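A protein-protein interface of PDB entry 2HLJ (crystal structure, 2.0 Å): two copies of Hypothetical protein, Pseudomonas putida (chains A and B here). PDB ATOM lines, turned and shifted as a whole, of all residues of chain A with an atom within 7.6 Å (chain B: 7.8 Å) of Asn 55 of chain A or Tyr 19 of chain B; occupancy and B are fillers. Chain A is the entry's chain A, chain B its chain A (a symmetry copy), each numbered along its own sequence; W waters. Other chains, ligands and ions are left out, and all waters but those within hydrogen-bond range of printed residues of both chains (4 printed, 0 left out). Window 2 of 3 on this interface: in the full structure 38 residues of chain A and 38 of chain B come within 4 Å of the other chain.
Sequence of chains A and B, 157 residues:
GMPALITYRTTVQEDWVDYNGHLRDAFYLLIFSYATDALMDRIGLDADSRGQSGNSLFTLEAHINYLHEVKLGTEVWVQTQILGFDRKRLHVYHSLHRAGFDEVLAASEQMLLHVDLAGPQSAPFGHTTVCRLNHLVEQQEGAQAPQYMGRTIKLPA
O of Arg 50 of chain A sits close to ND2 of Asn 55 of chain A (3.3 Å).
O of Gln 52 of chain A lies within hydrogen-bond range of ND2 of Asn 55 of chain A, 3.3 Å away.
The backbone NH (N) of Asn 20 of chain B sits at hydrogen-bond distance from the side-chain carboxylate (OD1) of Asp 18 of chain B (3.1 Å).
OD1 of Asp 18 of chain B sits at hydrogen-bond distance from N of Gly 21 of chain B.
The side-chain carboxylate (OD1) of Asp 18 of chain B is in hydrogen-bond range of the backbone NH (N) of His 22 of chain B, at 3.0 Å.
Among the printed residues, merely in contact across the chains: Arg 50 of chain A with Tyr 19 of chain B (3.2 Å), Arg 50 of chain A with Asn 20 of chain B (3.7 Å), Asn 55 of chain A with Asp 18 of chain B (3.2 Å), Asn 55 of chain A with Tyr 19 of chain B (3.5 Å) and Asn 55 of chain A with Asn 20 of chain B (3.9 Å).
No position is printed for both chains.
Of the 6 pairs that touch across the chains among the printed residues, none has its exchanged pair printed and touching as well.
Hydrophobic or aromatic side chains of chain B that line the printed part of chain A: Tyr 19.
Printed residues of chain A that touch a printed residue of chain B: Asp 37, Arg 50 and Asn 55.
Among the printed residues, 6 pairs touch across the chains.
Among the printed residues, Asp or Glu carboxylates within 4 Å of a Lys or Arg side-chain nitrogen of the other chain: Asp 37 of chain A with Arg 24 of chain B.
Water W3 bridges the side-chain carboxylate (OD2) of Asp 37 of chain A (2.5 Å) and the guanidinium group (NH2) of Arg 24 of chain B (3.4 Å).
Water W4 lies within hydrogen-bond range of the side-chain amide nitrogen (ND2) of Asn 20 of chain B, the backbone carbonyl oxygen (O) of Asn 55 of chain A and the side-chain carboxylate (OD2) of Asp 18 of chain B.
Water W1 bridges OD1 of Asn 20 of chain B (3.0 Å) and NH1 of Arg 50 of chain A (3.0 Å).
Water W2 bridges the backbone carbonyl oxygen of Leu 117 of chain A (3.3 Å) and the side-chain amide nitrogen of Asn 20 of chain B (3.4 Å).
Asn 55 of chain A touches just these residues of chain B: Asp 18 (3.2 Å), Tyr 19 (3.5 Å) and Asn 20 (3.9 Å).
Tyr 19 of chain B touches just these residues of chain A: Arg 50 and Asn 55.
No residue of chain B comes within 4 Å of Gly 54 of chain A.
Of the printed residues of chain A, Asp 18 of chain B touches Asn 55.
Of the printed residues of chain B, Arg 50 of chain A touches Tyr 19 and Asn 20.
Of the printed residues of chain A, Arg 24 of chain B touches Asp 37.
Of the printed residues of chain A, Asn 20 of chain B touches Arg 50 (3.7 Å) and Asn 55 (3.9 Å).
Of the printed residues of chain B, Asp 37 of chain A touches Arg 24.
Val 17 of chain B touches none of the printed residues of chain A.
Leu 117 of chain A touches none of the printed residues of chain B.
The nearest residue of chain B that does not touch Asn 55 of chain A is Arg 24 of chain B (5.6 Å).
The nearest printed residue of chain A that does not touch Tyr 19 of chain B is Ser 49 of chain A (6.6 Å).
NH1 of Arg 24 of chain B is in salt-bridge range of OD2 of Asp 37 of chain A (2.9 Å).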
ATOM      1  N   THR A  36      -3.502  -0.969  27.807  1.00  0.00           N
ATOM      2  CA  THR A  36      -2.137  -1.237  28.315  1.00  0.00           C
ATOM      3  C   THR A  36      -1.153  -0.229  27.722  1.00  0.00           C
ATOM      4  O   THR A  36      -0.335   0.351  28.432  1.00  0.00           O
ATOM      5  CB  THR A  36      -1.689  -2.660  27.959  1.00  0.00           C
ATOM      6  OG1 THR A  36      -2.545  -3.625  28.583  1.00  0.00           O
ATOM      7  CG2 THR A  36      -0.235  -2.917  28.400  1.00  0.00           C
ATOM      8  N   ASP A  37      -1.276   0.047  26.425  1.00  0.00           N
ATOM      9  CA  ASP A  37      -0.398   1.037  25.795  1.00  0.00           C
ATOM     10  C   ASP A  37      -0.557   2.454  26.419  1.00  0.00           C
ATOM     11  O   ASP A  37       0.415   3.170  26.696  1.00  0.00           O
ATOM     12  CB  ASP A  37      -0.628   1.102  24.288  1.00  0.00           C
ATOM     13  CG  ASP A  37      -0.299  -0.204  23.566  1.00  0.00           C
ATOM     14  OD1 ASP A  37       0.268  -1.146  24.163  1.00  0.00           O
ATOM     15  OD2 ASP A  37      -0.643  -0.292  22.375  1.00  0.00           O
ATOM     16  N   MET A  40       1.094   2.766  29.725  1.00  0.00           N
ATOM     17  CA  MET A  40       2.524   2.992  29.583  1.00  0.00           C
ATOM     18  C   MET A  40       2.823   4.431  29.177  1.00  0.00           C
ATOM     19  O   MET A  40       3.776   5.030  29.701  1.00  0.00           O
ATOM     20  CB  MET A  40       3.174   1.976  28.631  1.00  0.00           C
ATOM     21  CG  MET A  40       3.162   0.544  29.122  1.00  0.00           C
ATOM     22  SD  MET A  40       3.658   0.362  30.997  1.00  0.00           S
ATOM     23  CE  MET A  40       1.970  -0.194  31.758  1.00  0.00           C
ATOM     24  N   LEU A  45       6.731   5.132  30.196  1.00  0.00           N
ATOM     25  CA  LEU A  45       7.684   4.026  30.126  1.00  0.00           C
ATOM     26  C   LEU A  45       8.328   4.016  28.761  1.00  0.00           C
ATOM     27  O   LEU A  45       7.634   3.911  27.752  1.00  0.00           O
ATOM     28  CB  LEU A  45       7.023   2.692  30.395  1.00  0.00           C
ATOM     29  CG  LEU A  45       7.913   1.446  30.198  1.00  0.00           C
ATOM     30  CD1 LEU A  45       9.054   1.379  31.190  1.00  0.00           C
ATOM     31  CD2 LEU A  45       7.099   0.174  30.266  1.00  0.00           C
ATOM     32  N   ASP A  46       9.651   4.131  28.746  1.00  0.00           N
ATOM     33  CA  ASP A  46      10.445   4.158  27.508  1.00  0.00           C
ATOM     34  C   ASP A  46       9.928   5.181  26.504  1.00  0.00           C
ATOM     35  O   ASP A  46       9.976   4.950  25.309  1.00  0.00           O
ATOM     36  CB  ASP A  46      10.494   2.778  26.877  1.00  0.00           C
ATOM     37  CG  ASP A  46      11.174   1.757  27.757  1.00  0.00           C
ATOM     38  OD1 ASP A  46      12.307   2.015  28.232  1.00  0.00           O
ATOM     39  OD2 ASP A  46      10.586   0.680  27.956  1.00  0.00           O
ATOM     40  N   SER A  49      11.995   6.333  23.281  1.00  0.00           N
ATOM     41  CA  SER A  49      12.570   5.312  22.374  1.00  0.00           C
ATOM     42  C   SER A  49      11.470   4.565  21.619  1.00  0.00           C
ATOM     43  O   SER A  49      10.289   4.895  21.751  1.00  0.00           O
ATOM     44  CB  SER A  49      13.420   4.312  23.151  1.00  0.00           C
ATOM     45  OG  SER A  49      12.601   3.418  23.889  1.00  0.00           O
ATOM     46  N   ARG A  50      11.864   3.597  20.784  1.00  0.00           N
ATOM     47  CA  ARG A  50      10.874   2.742  20.119  1.00  0.00           C
ATOM     48  C   ARG A  50      10.133   1.822  21.086  1.00  0.00           C
ATOM     49  O   ARG A  50       9.171   1.162  20.686  1.00  0.00           O
ATOM     50  CB  ARG A  50      11.513   1.931  18.974  1.00  0.00           C
ATOM     51  CG  ARG A  50      12.039   2.808  17.835  1.00  0.00           C
ATOM     52  CD  ARG A  50      12.344   2.032  16.594  1.00  0.00           C
ATOM     53  NE  ARG A  50      12.711   2.932  15.485  1.00  0.00           N
ATOM     54  CZ  ARG A  50      12.867   2.550  14.220  1.00  0.00           C
ATOM     55  NH1 ARG A  50      12.685   1.287  13.869  1.00  0.00           N
ATOM     56  NH2 ARG A  50      13.179   3.446  13.292  1.00  0.00           N
ATOM     57  N   GLY A  51      10.564   1.733  22.343  1.00  0.00           N
ATOM     58  CA  GLY A  51       9.781   0.994  23.382  1.00  0.00           C
ATOM     59  C   GLY A  51       8.548   1.704  23.926  1.00  0.00           C
ATOM     60  O   GLY A  51       7.754   1.110  24.698  1.00  0.00           O
ATOM     61  N   GLN A  52       8.354   2.964  23.517  1.00  0.00           N
ATOM     62  CA  GLN A  52       7.251   3.791  24.010  1.00  0.00           C
ATOM     63  C   GLN A  52       5.881   3.132  23.793  1.00  0.00           C
ATOM     64  O   GLN A  52       5.732   2.244  22.947  1.00  0.00           O
ATOM     65  CB  GLN A  52       7.280   5.181  23.353  1.00  0.00           C
ATOM     66  CG  GLN A  52       7.065   5.206  21.850  1.00  0.00           C
ATOM     67  CD  GLN A  52       7.222   6.609  21.237  1.00  0.00           C
ATOM     68  OE1 GLN A  52       8.209   7.300  21.450  1.00  0.00           O
ATOM     69  NE2 GLN A  52       6.243   7.013  20.468  1.00  0.00           N
ATOM     70  N   SER A  53       4.903   3.553  24.590  1.00  0.00           N
ATOM     71  CA  SER A  53       3.494   3.261  24.355  1.00  0.00           C
ATOM     72  C   SER A  53       3.212   1.787  24.314  1.00  0.00           C
ATOM     73  O   SER A  53       2.461   1.331  23.464  1.00  0.00           O
ATOM     74  CB  SER A  53       3.039   3.919  23.046  1.00  0.00           C
ATOM     75  OG  SER A  53       3.241   5.301  23.093  1.00  0.00           O
ATOM     76  N   GLY A  54       3.809   1.034  25.244  1.00  0.00           N
ATOM     77  CA  GLY A  54       3.637  -0.388  25.287  1.00  0.00           C
ATOM     78  C   GLY A  54       4.537  -1.217  24.383  1.00  0.00           C
ATOM     79  O   GLY A  54       4.598  -2.424  24.537  1.00  0.00           O
ATOM     80  N   ASN A  55       5.277  -0.606  23.463  1.00  0.00           N
ATOM     81  CA  ASN A  55       6.108  -1.406  22.571  1.00  0.00           C
ATOM     82  C   ASN A  55       7.171  -2.238  23.292  1.00  0.00           C
ATOM     83  O   ASN A  55       7.572  -3.273  22.773  1.00  0.00           O
ATOM     84  CB  ASN A  55       6.755  -0.546  21.471  1.00  0.00           C
ATOM     85  CG  ASN A  55       5.750  -0.063  20.410  1.00  0.00           C
ATOM     86  OD1 ASN A  55       4.806  -0.760  20.069  1.00  0.00           O
ATOM     87  ND2 ASN A  55       5.980   1.127  19.870  1.00  0.00           N
ATOM     88  N   SER A  56       7.610  -1.821  24.476  1.00  0.00           N
ATOM     89  CA  SER A  56       8.632  -2.575  25.231  1.00  0.00           C
ATOM     90  C   SER A  56       8.024  -3.607  26.167  1.00  0.00           C
ATOM     91  O   SER A  56       8.732  -4.140  27.026  1.00  0.00           O
ATOM     92  CB  SER A  56       9.460  -1.621  26.100  1.00  0.00           C
ATOM     93  OG  SER A  56       8.591  -0.885  26.950  1.00  0.00           O
ATOM     94  N   LEU A  57       6.721  -3.864  26.062  1.00  0.00           N
ATOM     95  CA  LEU A  57       6.080  -4.893  26.886  1.00  0.00           C
ATOM     96  C   LEU A  57       5.667  -6.091  26.025  1.00  0.00           C
ATOM     97  O   LEU A  57       5.068  -5.915  24.978  1.00  0.00           O
ATOM     98  CB  LEU A  57       4.837  -4.338  27.555  1.00  0.00           C
ATOM     99  CG  LEU A  57       5.024  -3.266  28.606  1.00  0.00           C
ATOM    100  CD1 LEU A  57       3.673  -2.965  29.195  1.00  0.00           C
ATOM    101  CD2 LEU A  57       6.009  -3.697  29.693  1.00  0.00           C
ATOM    102  N   PHE A  58       5.971  -7.293  26.475  1.00  0.00           N
ATOM    103  CA  PHE A  58       5.495  -8.495  25.824  1.00  0.00           C
ATOM    104  C   PHE A  58       4.471  -9.114  26.768  1.00  0.00           C
ATOM    105  O   PHE A  58       4.771  -9.359  27.939  1.00  0.00           O
ATOM    106  CB  PHE A  58       6.670  -9.450  25.583  1.00  0.00           C
ATOM    107  CG  PHE A  58       6.285 -10.780  24.926  1.00  0.00           C
ATOM    108  CD1 PHE A  58       5.917 -10.838  23.579  1.00  0.00           C
ATOM    109  CD2 PHE A  58       6.299 -11.963  25.663  1.00  0.00           C
ATOM    110  CE1 PHE A  58       5.576 -12.062  22.977  1.00  0.00           C
ATOM    111  CE2 PHE A  58       5.966 -13.198  25.079  1.00  0.00           C
ATOM    112  CZ  PHE A  58       5.600 -13.251  23.737  1.00  0.00           C
ATOM    113  N   LEU A 113       5.787  -8.543  30.458  1.00  0.00           N
ATOM    114  CA  LEU A 113       7.237  -8.543  30.637  1.00  0.00           C
ATOM    115  C   LEU A 113       7.831  -7.327  29.956  1.00  0.00           C
ATOM    116  O   LEU A 113       7.528  -7.063  28.771  1.00  0.00           O
ATOM    117  CB  LEU A 113       7.849  -9.802  29.993  1.00  0.00           C
ATOM    118  CG  LEU A 113       9.381  -9.932  30.023  1.00  0.00           C
ATOM    119  CD1 LEU A 113       9.875 -10.015  31.442  1.00  0.00           C
ATOM    120  CD2 LEU A 113       9.857 -11.136  29.242  1.00  0.00           C
ATOM    121  N   HIS A 114       8.675  -6.593  30.688  1.00  0.00           N
ATOM    122  CA  HIS A 114       9.404  -5.478  30.103  1.00  0.00           C
ATOM    123  C   HIS A 114      10.621  -6.053  29.410  1.00  0.00           C
ATOM    124  O   HIS A 114      11.418  -6.760  30.014  1.00  0.00           O
ATOM    125  CB  HIS A 114       9.796  -4.442  31.166  1.00  0.00           C
ATOM    126  CG  HIS A 114      10.452  -3.200  30.620  1.00  0.00           C
ATOM    127  ND1 HIS A 114      11.569  -2.645  31.202  1.00  0.00           N
ATOM    128  CD2 HIS A 114      10.129  -2.386  29.582  1.00  0.00           C
ATOM    129  CE1 HIS A 114      11.924  -1.557  30.528  1.00  0.00           C
ATOM    130  NE2 HIS A 114      11.067  -1.375  29.543  1.00  0.00           N
ATOM    131  N   VAL A 115      10.764  -5.738  28.139  1.00  0.00           N
ATOM    132  CA  VAL A 115      11.796  -6.359  27.308  1.00  0.00           C
ATOM    133  C   VAL A 115      12.783  -5.317  26.812  1.00  0.00           C
ATOM    134  O   VAL A 115      12.412  -4.209  26.500  1.00  0.00           O
ATOM    135  CB  VAL A 115      11.204  -7.154  26.102  1.00  0.00           C
ATOM    136  CG1 VAL A 115      10.236  -8.191  26.579  1.00  0.00           C
ATOM    137  CG2 VAL A 115      10.528  -6.247  25.109  1.00  0.00           C
ATOM    138  N   LEU A 117      14.828  -3.753  24.036  1.00  0.00           N
ATOM    139  CA  LEU A 117      14.918  -3.613  22.577  1.00  0.00           C
ATOM    140  C   LEU A 117      14.000  -4.571  21.852  1.00  0.00           C
ATOM    141  O   LEU A 117      12.796  -4.381  21.894  1.00  0.00           O
ATOM    142  CB  LEU A 117      16.359  -3.819  22.088  1.00  0.00           C
ATOM    143  CG  LEU A 117      17.377  -2.871  22.725  1.00  0.00           C
ATOM    144  CD1 LEU A 117      18.790  -3.231  22.265  1.00  0.00           C
ATOM    145  CD2 LEU A 117      17.019  -1.391  22.443  1.00  0.00           C
ATOM    146  N   GLU B  14       0.965  -6.365   8.315  1.00  0.00           N
ATOM    147  CA  GLU B  14       1.479  -5.164   8.934  1.00  0.00           C
ATOM    148  C   GLU B  14       0.481  -4.497   9.876  1.00  0.00           C
ATOM    149  O   GLU B  14       0.902  -3.828  10.799  1.00  0.00           O
ATOM    150  CB  GLU B  14       1.919  -4.162   7.885  1.00  0.00           C
ATOM    151  CG  GLU B  14       2.876  -3.109   8.416  1.00  0.00           C
ATOM    152  CD  GLU B  14       3.565  -2.292   7.306  1.00  0.00           C
ATOM    153  OE1 GLU B  14       3.535  -2.708   6.123  1.00  0.00           O
ATOM    154  OE2 GLU B  14       4.141  -1.236   7.646  1.00  0.00           O
ATOM    155  N   VAL B  17       0.932  -5.800  13.764  1.00  0.00           N
ATOM    156  CA  VAL B  17       2.200  -5.725  14.428  1.00  0.00           C
ATOM    157  C   VAL B  17       2.446  -4.334  14.985  1.00  0.00           C
ATOM    158  O   VAL B  17       1.871  -3.372  14.520  1.00  0.00           O
ATOM    159  CB  VAL B  17       3.397  -6.207  13.550  1.00  0.00           C
ATOM    160  CG1 VAL B  17       3.129  -7.616  12.953  1.00  0.00           C
ATOM    161  CG2 VAL B  17       3.744  -5.232  12.466  1.00  0.00           C
ATOM    162  N   ASP B  18       3.287  -4.274  16.011  1.00  0.00           N
ATOM    163  CA  ASP B  18       3.679  -3.025  16.644  1.00  0.00           C
ATOM    164  C   ASP B  18       4.842  -2.429  15.843  1.00  0.00           C
ATOM    165  O   ASP B  18       5.216  -2.943  14.786  1.00  0.00           O
ATOM    166  CB  ASP B  18       4.029  -3.227  18.131  1.00  0.00           C
ATOM    167  CG  ASP B  18       5.126  -4.252  18.359  1.00  0.00           C
ATOM    168  OD1 ASP B  18       5.976  -4.449  17.463  1.00  0.00           O
ATOM    169  OD2 ASP B  18       5.148  -4.863  19.444  1.00  0.00           O
ATOM    170  N   TYR B  19       5.385  -1.324  16.339  1.00  0.00           N
ATOM    171  CA  TYR B  19       6.407  -0.566  15.643  1.00  0.00           C
ATOM    172  C   TYR B  19       7.634  -1.433  15.353  1.00  0.00           C
ATOM    173  O   TYR B  19       8.313  -1.253  14.341  1.00  0.00           O
ATOM    174  CB  TYR B  19       6.785   0.694  16.479  1.00  0.00           C
ATOM    175  CG  TYR B  19       7.496   1.768  15.677  1.00  0.00           C
ATOM    176  CD1 TYR B  19       6.846   2.469  14.658  1.00  0.00           C
ATOM    177  CD2 TYR B  19       8.826   2.087  15.931  1.00  0.00           C
ATOM    178  CE1 TYR B  19       7.533   3.461  13.907  1.00  0.00           C
ATOM    179  CE2 TYR B  19       9.491   3.072  15.198  1.00  0.00           C
ATOM    180  CZ  TYR B  19       8.855   3.741  14.196  1.00  0.00           C
ATOM    181  OH  TYR B  19       9.578   4.702  13.511  1.00  0.00           O
ATOM    182  N   ASN B  20       7.887  -2.388  16.241  1.00  0.00           N
ATOM    183  CA  ASN B  20       9.013  -3.288  16.146  1.00  0.00           C
ATOM    184  C   ASN B  20       8.760  -4.576  15.340  1.00  0.00           C
ATOM    185  O   ASN B  20       9.630  -5.425  15.205  1.00  0.00           O
ATOM    186  CB  ASN B  20       9.474  -3.589  17.554  1.00  0.00           C
ATOM    187  CG  ASN B  20       9.817  -2.304  18.334  1.00  0.00           C
ATOM    188  OD1 ASN B  20      10.151  -1.266  17.745  1.00  0.00           O
ATOM    189  ND2 ASN B  20       9.699  -2.364  19.647  1.00  0.00           N
ATOM    190  N   GLY B  21       7.573  -4.699  14.773  1.00  0.00           N
ATOM    191  CA  GLY B  21       7.275  -5.780  13.845  1.00  0.00           C
ATOM    192  C   GLY B  21       6.818  -7.047  14.533  1.00  0.00           C
ATOM    193  O   GLY B  21       6.782  -8.099  13.898  1.00  0.00           O
ATOM    194  N   HIS B  22       6.398  -6.933  15.797  1.00  0.00           N
ATOM    195  CA  HIS B  22       5.872  -8.095  16.528  1.00  0.00           C
ATOM    196  C   HIS B  22       4.355  -8.115  16.634  1.00  0.00           C
ATOM    197  O   HIS B  22       3.718  -7.104  16.921  1.00  0.00           O
ATOM    198  CB  HIS B  22       6.467  -8.173  17.910  1.00  0.00           C
ATOM    199  CG  HIS B  22       7.920  -8.506  17.899  1.00  0.00           C
ATOM    200  ND1 HIS B  22       8.792  -8.055  18.860  1.00  0.00           N
ATOM    201  CD2 HIS B  22       8.668  -9.187  16.998  1.00  0.00           C
ATOM    202  CE1 HIS B  22      10.009  -8.474  18.571  1.00  0.00           C
ATOM    203  NE2 HIS B  22       9.960  -9.174  17.455  1.00  0.00           N
ATOM    204  N   ARG B  24       0.888  -8.173  17.891  1.00  0.00           N
ATOM    205  CA  ARG B  24       0.242  -7.704  19.136  1.00  0.00           C
ATOM    206  C   ARG B  24      -0.556  -8.837  19.784  1.00  0.00           C
ATOM    207  O   ARG B  24      -1.129  -9.689  19.073  1.00  0.00           O
ATOM    208  CB  ARG B  24      -0.651  -6.484  18.842  1.00  0.00           C
ATOM    209  CG  ARG B  24      -1.452  -5.987  20.060  1.00  0.00           C
ATOM    210  CD  ARG B  24      -2.435  -4.917  19.659  1.00  0.00           C
ATOM    211  NE  ARG B  24      -1.769  -3.696  19.226  1.00  0.00           N
ATOM    212  CZ  ARG B  24      -1.266  -2.794  20.067  1.00  0.00           C
ATOM    213  NH1 ARG B  24      -1.328  -2.963  21.405  1.00  0.00           N
ATOM    214  NH2 ARG B  24      -0.677  -1.724  19.563  1.00  0.00           N
HETATM  215  O   HOH W   1      11.992  -1.222  15.434  1.00  0.00           O
HETATM  216  O   HOH W   2      13.024  -1.636  20.026  1.00  0.00           O
HETATM  217  O   HOH W   3      -1.503   1.385  20.712  1.00  0.00           O
HETATM  218  O   HOH W   4       7.666  -3.937  20.130  1.00  0.00           O
